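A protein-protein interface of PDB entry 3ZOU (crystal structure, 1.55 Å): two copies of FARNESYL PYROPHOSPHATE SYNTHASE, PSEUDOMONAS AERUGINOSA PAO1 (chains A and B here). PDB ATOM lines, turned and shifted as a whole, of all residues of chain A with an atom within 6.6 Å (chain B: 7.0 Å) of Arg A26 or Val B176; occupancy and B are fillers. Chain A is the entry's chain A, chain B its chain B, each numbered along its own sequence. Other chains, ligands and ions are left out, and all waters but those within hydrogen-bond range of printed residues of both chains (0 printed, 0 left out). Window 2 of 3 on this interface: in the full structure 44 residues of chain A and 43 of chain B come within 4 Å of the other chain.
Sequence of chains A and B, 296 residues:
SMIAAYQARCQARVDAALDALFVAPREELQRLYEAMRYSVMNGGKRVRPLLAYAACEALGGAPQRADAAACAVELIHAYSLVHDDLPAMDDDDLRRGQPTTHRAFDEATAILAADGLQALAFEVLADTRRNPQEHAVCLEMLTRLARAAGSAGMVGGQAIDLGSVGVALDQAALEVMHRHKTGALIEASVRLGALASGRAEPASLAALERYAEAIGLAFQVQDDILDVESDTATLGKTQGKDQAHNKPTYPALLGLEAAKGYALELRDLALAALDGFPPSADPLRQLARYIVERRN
Printed residues of chain B that touch a printed residue of chain A: Ala B152, Ile B160, Val B176 and His B180.
Of the 9 printed residues of chain A, 5 touch a printed residue of chain B.
Hydrophobic or aromatic side chains of chain A that line the printed part of chain B: Pro A25, Leu A29 and Tyr A33.
Among the printed residues, no Asp or Glu carboxylate lies within 4 Å of a Lys or Arg side-chain nitrogen of the other chain.
The backbone NH (N) of Ala B152 is in hydrogen-bond range of the side-chain hydroxyl (OH) of Tyr A33, 3.3 Å away.
Arg A26 touches just these residues of chain B: Val B176 and His B180.
Printed residues of chain A within 4 Å of Ala B152: Pro A25 and Tyr A33.
Val B176 touches just these residues of chain A: Arg A26 and Glu A28.
Met B177 touches none of the printed residues of chain A.
Of the printed residues of chain A, His B180 touches Arg A26.
The nearest printed residue of chain A that does not touch Val B176 is Leu A29 (7.3 Å).
The side-chain carboxylate of Glu A28 is in salt-bridge range of the guanidinium group of Arg A26 (2.9 Å).
O of Val B176 sits at hydrogen-bond distance from ND1 of His B180 (2.8 Å).
Among the printed residues, pairs that only touch across the chains: Arg A26 with Val B176 (3.7 Å), Leu A29 with Ile B160 (3.7 Å), Arg A26 with His B180 (3.7 Å), Glu A28 with Ile B160 (3.9 Å), Glu A28 with Val B176 (3.9 Å) and Pro A25 with Ala B152 (3.9 Å).
No position is printed for both chains.
Of the 7 pairs that touch across the chains among the printed residues, none has its exchanged pair printed and touching as well.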
ATOM      1  N   VAL A  23       5.097 -21.196  -0.035  1.00  0.00           N
ATOM      2  CA  VAL A  23       3.875 -20.770   0.654  1.00  0.00           C
ATOM      3  C   VAL A  23       4.070 -19.309   1.011  1.00  0.00           C
ATOM      4  O   VAL A  23       4.971 -18.944   1.736  1.00  0.00           O
ATOM      5  CB  VAL A  23       3.578 -21.637   1.910  1.00  0.00           C
ATOM      6  CG1 VAL A  23       2.315 -21.129   2.573  1.00  0.00           C
ATOM      7  CG2 VAL A  23       3.438 -23.116   1.556  1.00  0.00           C
ATOM      8  N   ALA A  24       3.216 -18.458   0.454  1.00  0.00           N
ATOM      9  CA  ALA A  24       3.282 -17.045   0.689  1.00  0.00           C
ATOM     10  C   ALA A  24       3.012 -16.748   2.138  1.00  0.00           C
ATOM     11  O   ALA A  24       2.071 -17.338   2.697  1.00  0.00           O
ATOM     12  CB  ALA A  24       2.251 -16.303  -0.165  1.00  0.00           C
ATOM     13  N   PRO A  25       3.812 -15.879   2.741  1.00  0.00           N
ATOM     14  CA  PRO A  25       3.554 -15.576   4.171  1.00  0.00           C
ATOM     15  C   PRO A  25       2.339 -14.700   4.419  1.00  0.00           C
ATOM     16  O   PRO A  25       1.898 -14.580   5.580  1.00  0.00           O
ATOM     17  CB  PRO A  25       4.821 -14.868   4.637  1.00  0.00           C
ATOM     18  CG  PRO A  25       5.576 -14.488   3.431  1.00  0.00           C
ATOM     19  CD  PRO A  25       5.069 -15.258   2.251  1.00  0.00           C
ATOM     20  N   ARG A  26       1.829 -14.078   3.384  1.00  0.00           N
ATOM     21  CA  ARG A  26       0.595 -13.293   3.476  1.00  0.00           C
ATOM     22  C   ARG A  26      -0.082 -13.198   2.141  1.00  0.00           C
ATOM     23  O   ARG A  26       0.524 -13.345   1.080  1.00  0.00           O
ATOM     24  CB  ARG A  26       0.866 -11.916   4.059  1.00  0.00           C
ATOM     25  CG  ARG A  26       1.864 -11.100   3.294  1.00  0.00           C
ATOM     26  CD  ARG A  26       2.336  -9.925   4.183  1.00  0.00           C
ATOM     27  NE  ARG A  26       1.189  -9.060   4.398  1.00  0.00           N
ATOM     28  CZ  ARG A  26       0.975  -8.250   5.442  1.00  0.00           C
ATOM     29  NH1 ARG A  26       1.852  -8.142   6.412  1.00  0.00           N
ATOM     30  NH2 ARG A  26      -0.165  -7.559   5.482  1.00  0.00           N
ATOM     31  N   GLU A  27      -1.359 -12.850   2.168  1.00  0.00           N
ATOM     32  CA  GLU A  27      -2.166 -12.877   0.986  1.00  0.00           C
ATOM     33  C   GLU A  27      -1.694 -11.971  -0.176  1.00  0.00           C
ATOM     34  O   GLU A  27      -1.821 -12.375  -1.323  1.00  0.00           O
ATOM     35  CB  GLU A  27      -3.589 -12.498   1.352  1.00  0.00           C
ATOM     36  CG  GLU A  27      -4.614 -12.784   0.285  1.00  0.00           C
ATOM     37  CD  GLU A  27      -6.033 -12.568   0.808  1.00  0.00           C
ATOM     38  OE1 GLU A  27      -6.165 -12.017   1.931  1.00  0.00           O
ATOM     39  OE2 GLU A  27      -6.995 -12.959   0.099  1.00  0.00           O
ATOM     40  N   GLU A  28      -1.117 -10.811   0.114  1.00  0.00           N
ATOM     41  CA  GLU A  28      -0.657  -9.911  -0.940  1.00  0.00           C
ATOM     42  C   GLU A  28       0.463 -10.478  -1.815  1.00  0.00           C
ATOM     43  O   GLU A  28       0.723  -9.991  -2.934  1.00  0.00           O
ATOM     44  CB  GLU A  28      -0.208  -8.566  -0.392  1.00  0.00           C
ATOM     45  CG  GLU A  28      -1.302  -7.851   0.453  1.00  0.00           C
ATOM     46  CD  GLU A  28      -1.268  -8.164   1.931  1.00  0.00           C
ATOM     47  OE1 GLU A  28      -0.957  -9.282   2.389  1.00  0.00           O
ATOM     48  OE2 GLU A  28      -1.600  -7.227   2.702  1.00  0.00           O
ATOM     49  N   LEU A  29       1.079 -11.510  -1.275  1.00  0.00           N
ATOM     50  CA  LEU A  29       2.245 -12.157  -1.941  1.00  0.00           C
ATOM     51  C   LEU A  29       1.883 -13.437  -2.629  1.00  0.00           C
ATOM     52  O   LEU A  29       2.735 -14.118  -3.190  1.00  0.00           O
ATOM     53  CB  LEU A  29       3.355 -12.372  -0.903  1.00  0.00           C
ATOM     54  CG  LEU A  29       3.943 -11.125  -0.216  1.00  0.00           C
ATOM     55  CD1 LEU A  29       4.894 -11.551   0.884  1.00  0.00           C
ATOM     56  CD2 LEU A  29       4.610 -10.175  -1.205  1.00  0.00           C
ATOM     57  N   GLN A  30       0.577 -13.800  -2.670  1.00  0.00           N
ATOM     58  CA  GLN A  30       0.189 -15.053  -3.245  1.00  0.00           C
ATOM     59  C   GLN A  30       0.597 -15.217  -4.683  1.00  0.00           C
ATOM     60  O   GLN A  30       1.083 -16.263  -5.079  1.00  0.00           O
ATOM     61  CB  GLN A  30      -1.331 -15.222  -3.126  1.00  0.00           C
ATOM     62  CG  GLN A  30      -1.639 -15.771  -1.756  1.00  0.00           C
ATOM     63  CD  GLN A  30      -3.108 -15.953  -1.497  1.00  0.00           C
ATOM     64  OE1 GLN A  30      -3.950 -15.369  -2.170  1.00  0.00           O
ATOM     65  NE2 GLN A  30      -3.414 -16.735  -0.473  1.00  0.00           N
ATOM     66  N   TYR A  33       4.379 -15.845  -5.163  1.00  0.00           N
ATOM     67  CA  TYR A  33       4.735 -17.210  -4.755  1.00  0.00           C
ATOM     68  C   TYR A  33       4.194 -18.210  -5.775  1.00  0.00           C
ATOM     69  O   TYR A  33       4.842 -19.228  -6.026  1.00  0.00           O
ATOM     70  CB  TYR A  33       4.311 -17.512  -3.331  1.00  0.00           C
ATOM     71  CG  TYR A  33       5.310 -16.985  -2.346  1.00  0.00           C
ATOM     72  CD1 TYR A  33       5.405 -15.614  -2.051  1.00  0.00           C
ATOM     73  CD2 TYR A  33       6.218 -17.832  -1.745  1.00  0.00           C
ATOM     74  CE1 TYR A  33       6.377 -15.133  -1.188  1.00  0.00           C
ATOM     75  CE2 TYR A  33       7.238 -17.345  -0.898  1.00  0.00           C
ATOM     76  CZ  TYR A  33       7.275 -15.996  -0.603  1.00  0.00           C
ATOM     77  OH  TYR A  33       8.251 -15.537   0.281  1.00  0.00           O
ATOM     78  N   ALA B 152       9.688 -12.617   0.564  1.00  0.00           N
ATOM     79  CA  ALA B 152       9.005 -12.185   1.770  1.00  0.00           C
ATOM     80  C   ALA B 152       9.390 -10.773   2.239  1.00  0.00           C
ATOM     81  O   ALA B 152       8.861 -10.319   3.268  1.00  0.00           O
ATOM     82  CB  ALA B 152       9.256 -13.190   2.846  1.00  0.00           C
ATOM     83  N   GLY B 157       7.798  -6.760  -1.808  1.00  0.00           N
ATOM     84  CA  GLY B 157       7.301  -5.378  -1.923  1.00  0.00           C
ATOM     85  C   GLY B 157       7.159  -4.912  -3.319  1.00  0.00           C
ATOM     86  O   GLY B 157       6.187  -4.250  -3.641  1.00  0.00           O
ATOM     87  N   ILE B 160       4.013  -6.488  -4.564  1.00  0.00           N
ATOM     88  CA  ILE B 160       2.826  -5.840  -3.996  1.00  0.00           C
ATOM     89  C   ILE B 160       2.609  -4.564  -4.730  1.00  0.00           C
ATOM     90  O   ILE B 160       1.430  -4.236  -5.045  1.00  0.00           O
ATOM     91  CB  ILE B 160       3.008  -5.568  -2.481  1.00  0.00           C
ATOM     92  CG1 ILE B 160       3.018  -6.888  -1.762  1.00  0.00           C
ATOM     93  CG2 ILE B 160       1.878  -4.693  -1.940  1.00  0.00           C
ATOM     94  CD1 ILE B 160       3.418  -6.788  -0.302  1.00  0.00           C
ATOM     95  N   ASP B 170      -5.311   2.348   0.678  1.00  0.00           N
ATOM     96  CA  ASP B 170      -5.471   3.208   1.819  1.00  0.00           C
ATOM     97  C   ASP B 170      -4.070   3.277   2.473  1.00  0.00           C
ATOM     98  O   ASP B 170      -3.092   2.643   1.983  1.00  0.00           O
ATOM     99  CB  ASP B 170      -6.599   2.747   2.785  1.00  0.00           C
ATOM    100  CG  ASP B 170      -6.457   1.328   3.298  1.00  0.00           C
ATOM    101  OD1 ASP B 170      -5.386   0.685   3.143  1.00  0.00           O
ATOM    102  OD2 ASP B 170      -7.404   0.863   3.966  1.00  0.00           O
ATOM    103  N   GLN B 171      -3.969   4.017   3.567  1.00  0.00           N
ATOM    104  CA  GLN B 171      -2.682   4.135   4.253  1.00  0.00           C
ATOM    105  C   GLN B 171      -2.147   2.762   4.700  1.00  0.00           C
ATOM    106  O   GLN B 171      -0.926   2.550   4.592  1.00  0.00           O
ATOM    107  CB  GLN B 171      -2.807   5.064   5.477  1.00  0.00           C
ATOM    108  CG  GLN B 171      -1.465   5.380   6.102  1.00  0.00           C
ATOM    109  CD  GLN B 171      -1.540   6.399   7.200  1.00  0.00           C
ATOM    110  OE1 GLN B 171      -2.511   7.193   7.255  1.00  0.00           O
ATOM    111  NE2 GLN B 171      -0.535   6.418   8.072  1.00  0.00           N
ATOM    112  N   ALA B 172      -2.993   1.891   5.233  1.00  0.00           N
ATOM    113  CA  ALA B 172      -2.542   0.616   5.780  1.00  0.00           C
ATOM    114  C   ALA B 172      -1.873  -0.188   4.658  1.00  0.00           C
ATOM    115  O   ALA B 172      -0.784  -0.751   4.827  1.00  0.00           O
ATOM    116  CB  ALA B 172      -3.663  -0.169   6.433  1.00  0.00           C
ATOM    117  N   ALA B 173      -2.491  -0.181   3.485  1.00  0.00           N
ATOM    118  CA  ALA B 173      -2.002  -0.987   2.366  1.00  0.00           C
ATOM    119  C   ALA B 173      -0.713  -0.358   1.825  1.00  0.00           C
ATOM    120  O   ALA B 173       0.246  -1.083   1.431  1.00  0.00           O
ATOM    121  CB  ALA B 173      -3.068  -1.129   1.296  1.00  0.00           C
ATOM    122  N   LEU B 174      -0.662   0.963   1.797  1.00  0.00           N
ATOM    123  CA  LEU B 174       0.520   1.669   1.375  1.00  0.00           C
ATOM    124  C   LEU B 174       1.699   1.327   2.304  1.00  0.00           C
ATOM    125  O   LEU B 174       2.817   1.111   1.818  1.00  0.00           O
ATOM    126  CB  LEU B 174       0.328   3.206   1.353  1.00  0.00           C
ATOM    127  CG  LEU B 174       1.514   4.071   0.894  1.00  0.00           C
ATOM    128  CD1 LEU B 174       1.878   3.738  -0.553  1.00  0.00           C
ATOM    129  CD2 LEU B 174       1.268   5.583   0.974  1.00  0.00           C
ATOM    130  N   GLU B 175       1.421   1.254   3.592  1.00  0.00           N
ATOM    131  CA  GLU B 175       2.466   0.956   4.573  1.00  0.00           C
ATOM    132  C   GLU B 175       2.931  -0.513   4.485  1.00  0.00           C
ATOM    133  O   GLU B 175       4.158  -0.778   4.633  1.00  0.00           O
ATOM    134  CB  GLU B 175       2.044   1.370   5.986  1.00  0.00           C
ATOM    135  CG  GLU B 175       2.060   2.877   6.024  1.00  0.00           C
ATOM    136  CD  GLU B 175       1.746   3.467   7.376  1.00  0.00           C
ATOM    137  OE1 GLU B 175       1.510   2.679   8.323  1.00  0.00           O
ATOM    138  OE2 GLU B 175       1.855   4.716   7.456  1.00  0.00           O
ATOM    139  N   VAL B 176       2.000  -1.414   4.223  1.00  0.00           N
ATOM    140  CA  VAL B 176       2.410  -2.853   3.988  1.00  0.00           C
ATOM    141  C   VAL B 176       3.399  -2.897   2.784  1.00  0.00           C
ATOM    142  O   VAL B 176       4.461  -3.525   2.857  1.00  0.00           O
ATOM    143  CB  VAL B 176       1.213  -3.740   3.691  1.00  0.00           C
ATOM    144  CG1 VAL B 176       1.661  -5.116   3.148  1.00  0.00           C
ATOM    145  CG2 VAL B 176       0.388  -3.950   4.953  1.00  0.00           C
ATOM    146  N   MET B 177       3.093  -2.163   1.729  1.00  0.00           N
ATOM    147  CA  MET B 177       3.939  -2.135   0.536  1.00  0.00           C
ATOM    148  C   MET B 177       5.310  -1.586   0.909  1.00  0.00           C
ATOM    149  O   MET B 177       6.340  -2.220   0.681  1.00  0.00           O
ATOM    150  CB  MET B 177       3.325  -1.286  -0.568  1.00  0.00           C
ATOM    151  CG  MET B 177       4.093  -1.385  -1.860  1.00  0.00           C
ATOM    152  SD  MET B 177       3.521  -0.237  -3.113  1.00  0.00           S
ATOM    153  CE  MET B 177       3.889   1.262  -2.176  1.00  0.00           C
ATOM    154  N   HIS B 178       5.321  -0.414   1.530  1.00  0.00           N
ATOM    155  CA  HIS B 178       6.582   0.220   1.886  1.00  0.00           C
ATOM    156  C   HIS B 178       7.406  -0.679   2.843  1.00  0.00           C
ATOM    157  O   HIS B 178       8.653  -0.756   2.703  1.00  0.00           O
ATOM    158  CB  HIS B 178       6.366   1.563   2.531  1.00  0.00           C
ATOM    159  CG  HIS B 178       6.029   2.640   1.567  1.00  0.00           C
ATOM    160  ND1 HIS B 178       6.574   2.752   0.317  1.00  0.00           N
ATOM    161  CD2 HIS B 178       5.239   3.737   1.729  1.00  0.00           C
ATOM    162  CE1 HIS B 178       6.069   3.819  -0.296  1.00  0.00           C
ATOM    163  NE2 HIS B 178       5.310   4.461   0.580  1.00  0.00           N
ATOM    164  N   ARG B 179       6.764  -1.288   3.828  1.00  0.00           N
ATOM    165  CA  ARG B 179       7.509  -2.090   4.801  1.00  0.00           C
ATOM    166  C   ARG B 179       8.246  -3.238   4.118  1.00  0.00           C
ATOM    167  O   ARG B 179       9.352  -3.596   4.545  1.00  0.00           O
ATOM    168  CB  ARG B 179       6.621  -2.583   5.944  1.00  0.00           C
ATOM    169  CG  ARG B 179       6.231  -1.477   6.932  1.00  0.00           C
ATOM    170  CD  ARG B 179       5.659  -2.049   8.231  1.00  0.00           C
ATOM    171  NE  ARG B 179       6.327  -3.256   8.774  1.00  0.00           N
ATOM    172  CZ  ARG B 179       7.605  -3.328   9.156  1.00  0.00           C
ATOM    173  NH1 ARG B 179       8.419  -2.278   9.018  1.00  0.00           N
ATOM    174  NH2 ARG B 179       8.062  -4.468   9.671  1.00  0.00           N
ATOM    175  N   HIS B 180       7.662  -3.800   3.060  1.00  0.00           N
ATOM    176  CA  HIS B 180       8.339  -4.862   2.301  1.00  0.00           C
ATOM    177  C   HIS B 180       9.354  -4.258   1.328  1.00  0.00           C
ATOM    178  O   HIS B 180      10.487  -4.668   1.312  1.00  0.00           O
ATOM    179  CB  HIS B 180       7.315  -5.661   1.497  1.00  0.00           C
ATOM    180  CG  HIS B 180       6.488  -6.553   2.328  1.00  0.00           C
ATOM    181  ND1 HIS B 180       5.426  -6.104   3.087  1.00  0.00           N
ATOM    182  CD2 HIS B 180       6.525  -7.897   2.478  1.00  0.00           C
ATOM    183  CE1 HIS B 180       4.910  -7.133   3.753  1.00  0.00           C
ATOM    184  NE2 HIS B 180       5.539  -8.233   3.376  1.00  0.00           N
ATOM    185  N   LYS B 181       8.939  -3.245   0.547  1.00  0.00           N
ATOM    186  CA  LYS B 181       9.726  -2.761  -0.600  1.00  0.00           C
ATOM    187  C   LYS B 181      10.984  -2.072  -0.194  1.00  0.00           C
ATOM    188  O   LYS B 181      12.034  -2.331  -0.758  1.00  0.00           O
ATOM    189  CB  LYS B 181       8.899  -1.832  -1.500  1.00  0.00           C
ATOM    190  CG  LYS B 181       9.590  -1.578  -2.807  1.00  0.00           C
ATOM    191  CD  LYS B 181       8.629  -0.936  -3.804  1.00  0.00           C
ATOM    192  CE  LYS B 181       8.474   0.503  -3.499  1.00  0.00           C
ATOM    193  NZ  LYS B 181       7.897   1.209  -4.693  1.00  0.00           N
ATOM    194  N   LEU B 217      10.091   4.093   7.464  1.00  0.00           N
ATOM    195  CA  LEU B 217       8.851   4.732   7.004  1.00  0.00           C
ATOM    196  C   LEU B 217       9.032   6.226   6.947  1.00  0.00           C
ATOM    197  O   LEU B 217       8.544   6.917   6.013  1.00  0.00           O
ATOM    198  CB  LEU B 217       7.698   4.348   7.894  1.00  0.00           C
ATOM    199  CG  LEU B 217       6.316   4.549   7.360  1.00  0.00           C
ATOM    200  CD1 LEU B 217       6.150   3.578   6.170  1.00  0.00           C
ATOM    201  CD2 LEU B 217       5.344   4.201   8.493  1.00  0.00           C
ATOM    202  N   TYR B 250       1.798  10.035   0.781  1.00  0.00           N
ATOM    203  CA  TYR B 250       1.378  10.432   2.125  1.00  0.00           C
ATOM    204  C   TYR B 250       0.650  11.791   2.159  1.00  0.00           C
ATOM    205  O   TYR B 250      -0.377  11.846   2.836  1.00  0.00           O
ATOM    206  CB  TYR B 250       2.541  10.346   3.137  1.00  0.00           C
ATOM    207  CG  TYR B 250       2.827   8.886   3.488  1.00  0.00           C
ATOM    208  CD1 TYR B 250       2.049   8.198   4.430  1.00  0.00           C
ATOM    209  CD2 TYR B 250       3.887   8.212   2.880  1.00  0.00           C
ATOM    210  CE1 TYR B 250       2.289   6.851   4.681  1.00  0.00           C
ATOM    211  CE2 TYR B 250       4.163   6.905   3.199  1.00  0.00           C
ATOM    212  CZ  TYR B 250       3.352   6.253   4.100  1.00  0.00           C
ATOM    213  OH  TYR B 250       3.583   4.933   4.442  1.00  0.00           O
